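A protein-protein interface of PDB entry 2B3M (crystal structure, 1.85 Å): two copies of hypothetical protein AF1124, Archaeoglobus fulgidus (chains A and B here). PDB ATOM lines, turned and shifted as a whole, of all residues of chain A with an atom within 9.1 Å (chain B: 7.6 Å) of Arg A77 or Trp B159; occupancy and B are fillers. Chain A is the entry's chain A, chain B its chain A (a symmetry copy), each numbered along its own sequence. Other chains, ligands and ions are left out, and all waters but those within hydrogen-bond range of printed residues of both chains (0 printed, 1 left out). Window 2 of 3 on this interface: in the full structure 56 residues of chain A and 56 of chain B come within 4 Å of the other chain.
ND2 of Asn A64 lies close to N of Val A66, at 3.3 Å. The side-chain hydroxyl (OG1) of Thr A76 lies close to the backbone NH (N) of Phe A78. The backbone carbonyl oxygen (O) of Ala A73 sits at hydrogen-bond distance from the side-chain hydroxyl (OG1) of Thr A76 (2.8 Å). N of Val B104 sits at hydrogen-bond distance from O of Leu B157 (2.9 Å). O of Thr B102 is in hydrogen-bond range of N of Trp B159 (2.9 Å). The backbone carbonyl oxygen of Phe A78 lies within hydrogen-bond range of the guanidinium group of Arg A117 (2.7 Å).
Arg A77 touches just one residue of chain B: Trp B159 (3.4 Å). Trp B159 touches just these residues of chain A: Thr A76 (3.9 Å), Arg A77 (3.4 Å) and Phe A78 (3.9 Å). Of the printed residues of chain B, Asn A64 touches Val B103. Printed residues of chain B within 4 Å of Phe A72: Thr B102. Of the printed residues of chain A, Val B103 touches Asn A64. Of the printed residues of chain A, Val B104 touches Phe A78 (3.6 Å). Printed residues of chain B within 4 Å of Thr A76: Trp B159 (3.9 Å). Lys A75 touches none of the printed residues of chain B. Pro B100 touches none of the printed residues of chain A. The nearest residue of chain B that does not touch Arg A77 is Asn B134 (6.0 Å). The nearest residue of chain A that does not touch Trp B159 is Val A66 (5.2 Å).
The side-chain amide oxygen (OD1) of Asn A64 sits close to the backbone carbonyl oxygen (O) of Val B103 (3.0 Å).
Along chain B the printed residues that touch a printed residue of chain A span positions 102 to 159. Of the 15 printed residues of chain A, 5 touch a printed residue of chain B. Among the printed residues, no Asp or Glu carboxylate lies within 4 Å of a Lys or Arg side-chain nitrogen of the other chain.
No position is printed for both chains. Of the 6 pairs that touch across the chains among the printed residues, none has its exchanged pair printed and touching as well.
Among the printed residues, merely in contact across the chains: Phe A72 with Thr B102, Thr A76 with Trp B159, Arg A77 with Trp B159, Phe A78 with Val B104 and Phe A78 with Trp B159.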
ATOM      1  N   ASN A  64      -6.514   1.269 -20.895  1.00  0.00           N
ATOM      2  CA  ASN A  64      -5.802  -0.025 -20.668  1.00  0.00           C
ATOM      3  C   ASN A  64      -4.461  -0.029 -21.430  1.00  0.00           C
ATOM      4  O   ASN A  64      -4.445   0.123 -22.656  1.00  0.00           O
ATOM      5  CB  ASN A  64      -6.730  -1.120 -21.205  1.00  0.00           C
ATOM      6  CG  ASN A  64      -6.350  -2.547 -20.815  1.00  0.00           C
ATOM      7  OD1 ASN A  64      -7.202  -3.449 -20.931  1.00  0.00           O
ATOM      8  ND2 ASN A  64      -5.108  -2.783 -20.446  1.00  0.00           N
ATOM      9  N   VAL A  66      -2.603  -2.195 -22.528  1.00  0.00           N
ATOM     10  CA  VAL A  66      -2.497  -3.175 -23.592  1.00  0.00           C
ATOM     11  C   VAL A  66      -2.873  -2.595 -24.967  1.00  0.00           C
ATOM     12  O   VAL A  66      -2.468  -3.135 -25.988  1.00  0.00           O
ATOM     13  CB  VAL A  66      -3.307  -4.468 -23.257  1.00  0.00           C
ATOM     14  CG1 VAL A  66      -4.831  -4.305 -23.587  1.00  0.00           C
ATOM     15  CG2 VAL A  66      -2.709  -5.677 -23.974  1.00  0.00           C
ATOM     16  N   PHE A  72       4.841  -2.435 -22.695  1.00  0.00           N
ATOM     17  CA  PHE A  72       3.935  -3.205 -21.843  1.00  0.00           C
ATOM     18  C   PHE A  72       3.248  -4.300 -22.638  1.00  0.00           C
ATOM     19  O   PHE A  72       3.270  -5.459 -22.236  1.00  0.00           O
ATOM     20  CB  PHE A  72       2.871  -2.303 -21.204  1.00  0.00           C
ATOM     21  CG  PHE A  72       1.822  -3.059 -20.420  1.00  0.00           C
ATOM     22  CD1 PHE A  72       0.662  -3.519 -21.040  1.00  0.00           C
ATOM     23  CD2 PHE A  72       2.014  -3.334 -19.066  1.00  0.00           C
ATOM     24  CE1 PHE A  72      -0.302  -4.225 -20.325  1.00  0.00           C
ATOM     25  CE2 PHE A  72       1.056  -4.049 -18.339  1.00  0.00           C
ATOM     26  CZ  PHE A  72      -0.109  -4.487 -18.975  1.00  0.00           C
ATOM     27  N   ALA A  73       2.636  -3.934 -23.768  1.00  0.00           N
ATOM     28  CA  ALA A  73       1.868  -4.910 -24.544  1.00  0.00           C
ATOM     29  C   ALA A  73       2.755  -6.010 -25.136  1.00  0.00           C
ATOM     30  O   ALA A  73       2.326  -7.154 -25.295  1.00  0.00           O
ATOM     31  CB  ALA A  73       1.078  -4.225 -25.651  1.00  0.00           C
ATOM     32  N   SER A  74       3.989  -5.656 -25.479  1.00  0.00           N
ATOM     33  CA  SER A  74       4.887  -6.643 -26.077  1.00  0.00           C
ATOM     34  C   SER A  74       5.258  -7.794 -25.091  1.00  0.00           C
ATOM     35  O   SER A  74       5.623  -8.887 -25.518  1.00  0.00           O
ATOM     36  CB  SER A  74       6.149  -5.971 -26.629  1.00  0.00           C
ATOM     37  OG  SER A  74       7.033  -5.668 -25.576  1.00  0.00           O
ATOM     38  N   LYS A  75       5.147  -7.535 -23.793  1.00  0.00           N
ATOM     39  CA  LYS A  75       5.423  -8.539 -22.763  1.00  0.00           C
ATOM     40  C   LYS A  75       4.238  -9.459 -22.440  1.00  0.00           C
ATOM     41  O   LYS A  75       4.418 -10.486 -21.748  1.00  0.00           O
ATOM     42  CB  LYS A  75       5.932  -7.851 -21.499  1.00  0.00           C
ATOM     43  CG  LYS A  75       7.223  -7.086 -21.739  1.00  0.00           C
ATOM     44  CD  LYS A  75       7.462  -6.008 -20.696  1.00  0.00           C
ATOM     45  CE  LYS A  75       8.833  -5.389 -20.925  1.00  0.00           C
ATOM     46  NZ  LYS A  75       9.328  -4.634 -19.742  1.00  0.00           N
ATOM     47  N   THR A  76       3.053  -9.114 -22.959  1.00  0.00           N
ATOM     48  CA  THR A  76       1.846  -9.906 -22.742  1.00  0.00           C
ATOM     49  C   THR A  76       1.788 -11.030 -23.761  1.00  0.00           C
ATOM     50  O   THR A  76       2.586 -11.057 -24.702  1.00  0.00           O
ATOM     51  CB  THR A  76       0.553  -9.071 -22.885  1.00  0.00           C
ATOM     52  OG1 THR A  76       0.275  -8.809 -24.277  1.00  0.00           O
ATOM     53  CG2 THR A  76       0.642  -7.758 -22.094  1.00  0.00           C
ATOM     54  N   ARG A  77       0.805 -11.922 -23.593  1.00  0.00           N
ATOM     55  CA  ARG A  77       0.601 -13.056 -24.510  1.00  0.00           C
ATOM     56  C   ARG A  77       0.272 -12.603 -25.929  1.00  0.00           C
ATOM     57  O   ARG A  77       0.507 -13.338 -26.881  1.00  0.00           O
ATOM     58  CB  ARG A  77      -0.493 -13.989 -23.978  1.00  0.00           C
ATOM     59  CG  ARG A  77       0.033 -14.910 -22.884  1.00  0.00           C
ATOM     60  CD  ARG A  77      -1.072 -15.606 -22.127  1.00  0.00           C
ATOM     61  NE  ARG A  77      -0.534 -16.513 -21.115  1.00  0.00           N
ATOM     62  CZ  ARG A  77      -0.167 -16.149 -19.885  1.00  0.00           C
ATOM     63  NH1 ARG A  77      -0.267 -14.880 -19.485  1.00  0.00           N
ATOM     64  NH2 ARG A  77       0.316 -17.061 -19.047  1.00  0.00           N
ATOM     65  N   PHE A  78      -0.254 -11.382 -26.063  1.00  0.00           N
ATOM     66  CA  PHE A  78      -0.494 -10.790 -27.388  1.00  0.00           C
ATOM     67  C   PHE A  78       0.770 -10.411 -28.143  1.00  0.00           C
ATOM     68  O   PHE A  78       0.745 -10.323 -29.373  1.00  0.00           O
ATOM     69  CB  PHE A  78      -1.352  -9.542 -27.258  1.00  0.00           C
ATOM     70  CG  PHE A  78      -2.811  -9.838 -27.074  1.00  0.00           C
ATOM     71  CD1 PHE A  78      -3.408 -10.912 -27.738  1.00  0.00           C
ATOM     72  CD2 PHE A  78      -3.590  -9.010 -26.275  1.00  0.00           C
ATOM     73  CE1 PHE A  78      -4.784 -11.178 -27.570  1.00  0.00           C
ATOM     74  CE2 PHE A  78      -4.959  -9.246 -26.121  1.00  0.00           C
ATOM     75  CZ  PHE A  78      -5.548 -10.347 -26.769  1.00  0.00           C
ATOM     76  N   GLY A  79       1.870 -10.180 -27.423  1.00  0.00           N
ATOM     77  CA  GLY A  79       3.131  -9.814 -28.072  1.00  0.00           C
ATOM     78  C   GLY A  79       3.105  -8.471 -28.801  1.00  0.00           C
ATOM     79  O   GLY A  79       3.889  -8.245 -29.724  1.00  0.00           O
ATOM     80  N   GLY A  80       2.233  -7.568 -28.369  1.00  0.00           N
ATOM     81  CA  GLY A  80       2.136  -6.234 -28.973  1.00  0.00           C
ATOM     82  C   GLY A  80       0.741  -5.670 -28.725  1.00  0.00           C
ATOM     83  O   GLY A  80      -0.141  -6.383 -28.246  1.00  0.00           O
ATOM     84  N   ARG A  81       0.543  -4.398 -29.056  1.00  0.00           N
ATOM     85  CA  ARG A  81      -0.727  -3.728 -28.722  1.00  0.00           C
ATOM     86  C   ARG A  81      -1.858  -4.305 -29.532  1.00  0.00           C
ATOM     87  O   ARG A  81      -1.661  -4.772 -30.652  1.00  0.00           O
ATOM     88  CB  ARG A  81      -0.630  -2.213 -28.965  1.00  0.00           C
ATOM     89  CG  ARG A  81       0.313  -1.531 -27.980  1.00  0.00           C
ATOM     90  CD  ARG A  81       0.483  -0.062 -28.362  1.00  0.00           C
ATOM     91  NE  ARG A  81       0.999   0.097 -29.723  1.00  0.00           N
ATOM     92  CZ  ARG A  81       1.445   1.244 -30.217  1.00  0.00           C
ATOM     93  NH1 ARG A  81       1.424   2.344 -29.463  1.00  0.00           N
ATOM     94  NH2 ARG A  81       1.897   1.296 -31.462  1.00  0.00           N
ATOM     95  N   VAL A  82      -3.049  -4.254 -28.958  1.00  0.00           N
ATOM     96  CA  VAL A  82      -4.244  -4.669 -29.676  1.00  0.00           C
ATOM     97  C   VAL A  82      -5.272  -3.538 -29.537  1.00  0.00           C
ATOM     98  O   VAL A  82      -5.272  -2.803 -28.536  1.00  0.00           O
ATOM     99  CB  VAL A  82      -4.847  -6.008 -29.137  1.00  0.00           C
ATOM    100  CG1 VAL A  82      -3.809  -7.144 -29.193  1.00  0.00           C
ATOM    101  CG2 VAL A  82      -5.463  -5.865 -27.728  1.00  0.00           C
ATOM    102  N   PRO A 115      -7.003 -11.037 -32.076  1.00  0.00           N
ATOM    103  CA  PRO A 115      -6.771  -9.616 -31.875  1.00  0.00           C
ATOM    104  C   PRO A 115      -6.745  -8.780 -33.166  1.00  0.00           C
ATOM    105  O   PRO A 115      -6.381  -9.279 -34.242  1.00  0.00           O
ATOM    106  CB  PRO A 115      -5.395  -9.577 -31.181  1.00  0.00           C
ATOM    107  CG  PRO A 115      -4.753 -10.865 -31.518  1.00  0.00           C
ATOM    108  CD  PRO A 115      -5.837 -11.868 -31.669  1.00  0.00           C
ATOM    109  N   ARG A 117      -4.867  -5.477 -34.698  1.00  0.00           N
ATOM    110  CA  ARG A 117      -3.677  -4.671 -34.444  1.00  0.00           C
ATOM    111  C   ARG A 117      -3.894  -3.225 -34.871  1.00  0.00           C
ATOM    112  O   ARG A 117      -4.710  -2.957 -35.763  1.00  0.00           O
ATOM    113  CB  ARG A 117      -2.495  -5.274 -35.210  1.00  0.00           C
ATOM    114  CG  ARG A 117      -2.217  -6.746 -34.808  1.00  0.00           C
ATOM    115  CD  ARG A 117      -1.687  -6.850 -33.381  1.00  0.00           C
ATOM    116  NE  ARG A 117      -1.478  -8.242 -32.959  1.00  0.00           N
ATOM    117  CZ  ARG A 117      -1.043  -8.613 -31.760  1.00  0.00           C
ATOM    118  NH1 ARG A 117      -0.734  -7.692 -30.848  1.00  0.00           N
ATOM    119  NH2 ARG A 117      -0.846  -9.909 -31.497  1.00  0.00           N
ATOM    120  N   LEU B  99     -10.055  -3.607 -13.574  1.00  0.00           N
ATOM    121  CA  LEU B  99      -9.927  -4.711 -12.630  1.00  0.00           C
ATOM    122  C   LEU B  99      -8.441  -5.050 -12.478  1.00  0.00           C
ATOM    123  O   LEU B  99      -7.678  -4.880 -13.422  1.00  0.00           O
ATOM    124  CB  LEU B  99     -10.708  -5.940 -13.099  1.00  0.00           C
ATOM    125  CG  LEU B  99     -12.238  -5.743 -13.294  1.00  0.00           C
ATOM    126  CD1 LEU B  99     -12.795  -6.880 -14.097  1.00  0.00           C
ATOM    127  CD2 LEU B  99     -12.961  -5.650 -11.950  1.00  0.00           C
ATOM    128  N   PRO B 100      -8.039  -5.525 -11.287  1.00  0.00           N
ATOM    129  CA  PRO B 100      -6.647  -5.920 -11.061  1.00  0.00           C
ATOM    130  C   PRO B 100      -6.161  -6.935 -12.108  1.00  0.00           C
ATOM    131  O   PRO B 100      -6.843  -7.914 -12.403  1.00  0.00           O
ATOM    132  CB  PRO B 100      -6.680  -6.563  -9.662  1.00  0.00           C
ATOM    133  CG  PRO B 100      -7.929  -6.085  -9.017  1.00  0.00           C
ATOM    134  CD  PRO B 100      -8.893  -5.704 -10.095  1.00  0.00           C
ATOM    135  N   GLY B 101      -4.962  -6.723 -12.638  1.00  0.00           N
ATOM    136  CA  GLY B 101      -4.405  -7.631 -13.632  1.00  0.00           C
ATOM    137  C   GLY B 101      -4.461  -7.027 -15.023  1.00  0.00           C
ATOM    138  O   GLY B 101      -4.861  -5.879 -15.189  1.00  0.00           O
ATOM    139  N   THR B 102      -4.010  -7.777 -16.025  1.00  0.00           N
ATOM    140  CA  THR B 102      -4.110  -7.304 -17.413  1.00  0.00           C
ATOM    141  C   THR B 102      -5.384  -7.886 -17.972  1.00  0.00           C
ATOM    142  O   THR B 102      -5.538  -9.105 -18.031  1.00  0.00           O
ATOM    143  CB  THR B 102      -2.914  -7.782 -18.256  1.00  0.00           C
ATOM    144  OG1 THR B 102      -1.698  -7.318 -17.653  1.00  0.00           O
ATOM    145  CG2 THR B 102      -3.005  -7.224 -19.681  1.00  0.00           C
ATOM    146  N   VAL B 103      -6.284  -7.016 -18.407  1.00  0.00           N
ATOM    147  CA  VAL B 103      -7.637  -7.450 -18.709  1.00  0.00           C
ATOM    148  C   VAL B 103      -7.838  -7.399 -20.226  1.00  0.00           C
ATOM    149  O   VAL B 103      -7.456  -6.408 -20.852  1.00  0.00           O
ATOM    150  CB  VAL B 103      -8.674  -6.572 -17.987  1.00  0.00           C
ATOM    151  CG1 VAL B 103     -10.095  -7.000 -18.375  1.00  0.00           C
ATOM    152  CG2 VAL B 103      -8.504  -6.661 -16.450  1.00  0.00           C
ATOM    153  N   VAL B 104      -8.418  -8.466 -20.790  1.00  0.00           N
ATOM    154  CA  VAL B 104      -8.717  -8.540 -22.230  1.00  0.00           C
ATOM    155  C   VAL B 104     -10.182  -8.926 -22.388  1.00  0.00           C
ATOM    156  O   VAL B 104     -10.620  -9.877 -21.770  1.00  0.00           O
ATOM    157  CB  VAL B 104      -7.840  -9.639 -22.897  1.00  0.00           C
ATOM    158  CG1 VAL B 104      -8.139  -9.717 -24.395  1.00  0.00           C
ATOM    159  CG2 VAL B 104      -6.344  -9.370 -22.634  1.00  0.00           C
ATOM    160  N   LEU B 106     -13.288 -10.794 -23.857  1.00  0.00           N
ATOM    161  CA  LEU B 106     -13.527 -11.991 -24.662  1.00  0.00           C
ATOM    162  C   LEU B 106     -14.936 -12.042 -25.300  1.00  0.00           C
ATOM    163  O   LEU B 106     -15.072 -12.528 -26.419  1.00  0.00           O
ATOM    164  CB  LEU B 106     -13.387 -13.269 -23.826  1.00  0.00           C
ATOM    165  CG  LEU B 106     -11.990 -13.582 -23.258  1.00  0.00           C
ATOM    166  CD1 LEU B 106     -12.071 -14.916 -22.540  1.00  0.00           C
ATOM    167  CD2 LEU B 106     -10.980 -13.637 -24.375  1.00  0.00           C
ATOM    168  N   ASN B 134      -8.747 -18.325 -15.556  1.00  0.00           N
ATOM    169  CA  ASN B 134      -8.614 -16.856 -15.475  1.00  0.00           C
ATOM    170  C   ASN B 134      -9.648 -16.100 -16.320  1.00  0.00           C
ATOM    171  O   ASN B 134      -9.424 -14.948 -16.675  1.00  0.00           O
ATOM    172  CB  ASN B 134      -7.224 -16.421 -15.913  1.00  0.00           C
ATOM    173  CG  ASN B 134      -6.895 -16.846 -17.340  1.00  0.00           C
ATOM    174  OD1 ASN B 134      -7.518 -17.759 -17.911  1.00  0.00           O
ATOM    175  ND2 ASN B 134      -5.887 -16.194 -17.918  1.00  0.00           N
ATOM    176  N   TYR B 136     -13.322 -14.512 -16.390  1.00  0.00           N
ATOM    177  CA  TYR B 136     -14.286 -13.989 -15.427  1.00  0.00           C
ATOM    178  C   TYR B 136     -15.552 -13.581 -16.176  1.00  0.00           C
ATOM    179  O   TYR B 136     -15.448 -12.813 -17.116  1.00  0.00           O
ATOM    180  CB  TYR B 136     -13.692 -12.755 -14.763  1.00  0.00           C
ATOM    181  CG  TYR B 136     -12.587 -13.112 -13.798  1.00  0.00           C
ATOM    182  CD1 TYR B 136     -11.320 -13.505 -14.274  1.00  0.00           C
ATOM    183  CD2 TYR B 136     -12.821 -13.129 -12.431  1.00  0.00           C
ATOM    184  CE1 TYR B 136     -10.292 -13.906 -13.382  1.00  0.00           C
ATOM    185  CE2 TYR B 136     -11.785 -13.502 -11.529  1.00  0.00           C
ATOM    186  CZ  TYR B 136     -10.546 -13.875 -12.017  1.00  0.00           C
ATOM    187  OH  TYR B 136      -9.557 -14.278 -11.114  1.00  0.00           O
ATOM    188  N   VAL B 156     -14.225 -11.667 -19.490  1.00  0.00           N
ATOM    189  CA  VAL B 156     -12.904 -11.154 -19.747  1.00  0.00           C
ATOM    190  C   VAL B 156     -11.863 -12.217 -19.341  1.00  0.00           C
ATOM    191  O   VAL B 156     -12.152 -13.069 -18.506  1.00  0.00           O
ATOM    192  CB  VAL B 156     -12.610  -9.845 -18.975  1.00  0.00           C
ATOM    193  CG1 VAL B 156     -13.537  -8.705 -19.396  1.00  0.00           C
ATOM    194  CG2 VAL B 156     -12.683 -10.043 -17.428  1.00  0.00           C
ATOM    195  N   LEU B 157     -10.707 -12.122 -19.970  1.00  0.00           N
ATOM    196  CA  LEU B 157      -9.496 -12.891 -19.609  1.00  0.00           C
ATOM    197  C   LEU B 157      -8.630 -11.973 -18.779  1.00  0.00           C
ATOM    198  O   LEU B 157      -8.467 -10.802 -19.144  1.00  0.00           O
ATOM    199  CB  LEU B 157      -8.747 -13.203 -20.900  1.00  0.00           C
ATOM    200  CG  LEU B 157      -8.603 -14.619 -21.400  1.00  0.00           C
ATOM    201  CD1 LEU B 157      -7.564 -14.604 -22.512  1.00  0.00           C
ATOM    202  CD2 LEU B 157      -8.102 -15.472 -20.264  1.00  0.00           C
ATOM    203  N   ILE B 158      -8.058 -12.470 -17.672  1.00  0.00           N
ATOM    204  CA  ILE B 158      -7.231 -11.609 -16.846  1.00  0.00           C
ATOM    205  C   ILE B 158      -5.896 -12.331 -16.597  1.00  0.00           C
ATOM    206  O   ILE B 158      -5.867 -13.476 -16.129  1.00  0.00           O
ATOM    207  CB  ILE B 158      -7.938 -11.170 -15.520  1.00  0.00           C
ATOM    208  CG1 ILE B 158      -9.281 -10.489 -15.799  1.00  0.00           C
ATOM    209  CG2 ILE B 158      -7.047 -10.204 -14.733  1.00  0.00           C
ATOM    210  CD1 ILE B 158     -10.002 -10.005 -14.518  1.00  0.00           C
ATOM    211  N   TRP B 159      -4.824 -11.665 -16.995  1.00  0.00           N
ATOM    212  CA  TRP B 159      -3.458 -12.201 -16.882  1.00  0.00           C
ATOM    213  C   TRP B 159      -2.814 -11.557 -15.670  1.00  0.00           C
ATOM    214  O   TRP B 159      -2.950 -10.369 -15.412  1.00  0.00           O
ATOM    215  CB  TRP B 159      -2.670 -11.863 -18.144  1.00  0.00           C
ATOM    216  CG  TRP B 159      -3.120 -12.592 -19.384  1.00  0.00           C
ATOM    217  CD1 TRP B 159      -3.523 -13.895 -19.468  1.00  0.00           C
ATOM    218  CD2 TRP B 159      -3.170 -12.070 -20.726  1.00  0.00           C
ATOM    219  NE1 TRP B 159      -3.862 -14.206 -20.765  1.00  0.00           N
ATOM    220  CE2 TRP B 159      -3.642 -13.113 -21.562  1.00  0.00           C
ATOM    221  CE3 TRP B 159      -2.873 -10.817 -21.300  1.00  0.00           C
ATOM    222  CZ2 TRP B 159      -3.820 -12.949 -22.956  1.00  0.00           C
ATOM    223  CZ3 TRP B 159      -3.036 -10.654 -22.690  1.00  0.00           C
ATOM    224  CH2 TRP B 159      -3.504 -11.723 -23.499  1.00  0.00           C
ATOM    225  OXT TRP B 159      -2.109 -12.207 -14.885  1.00  0.00           O
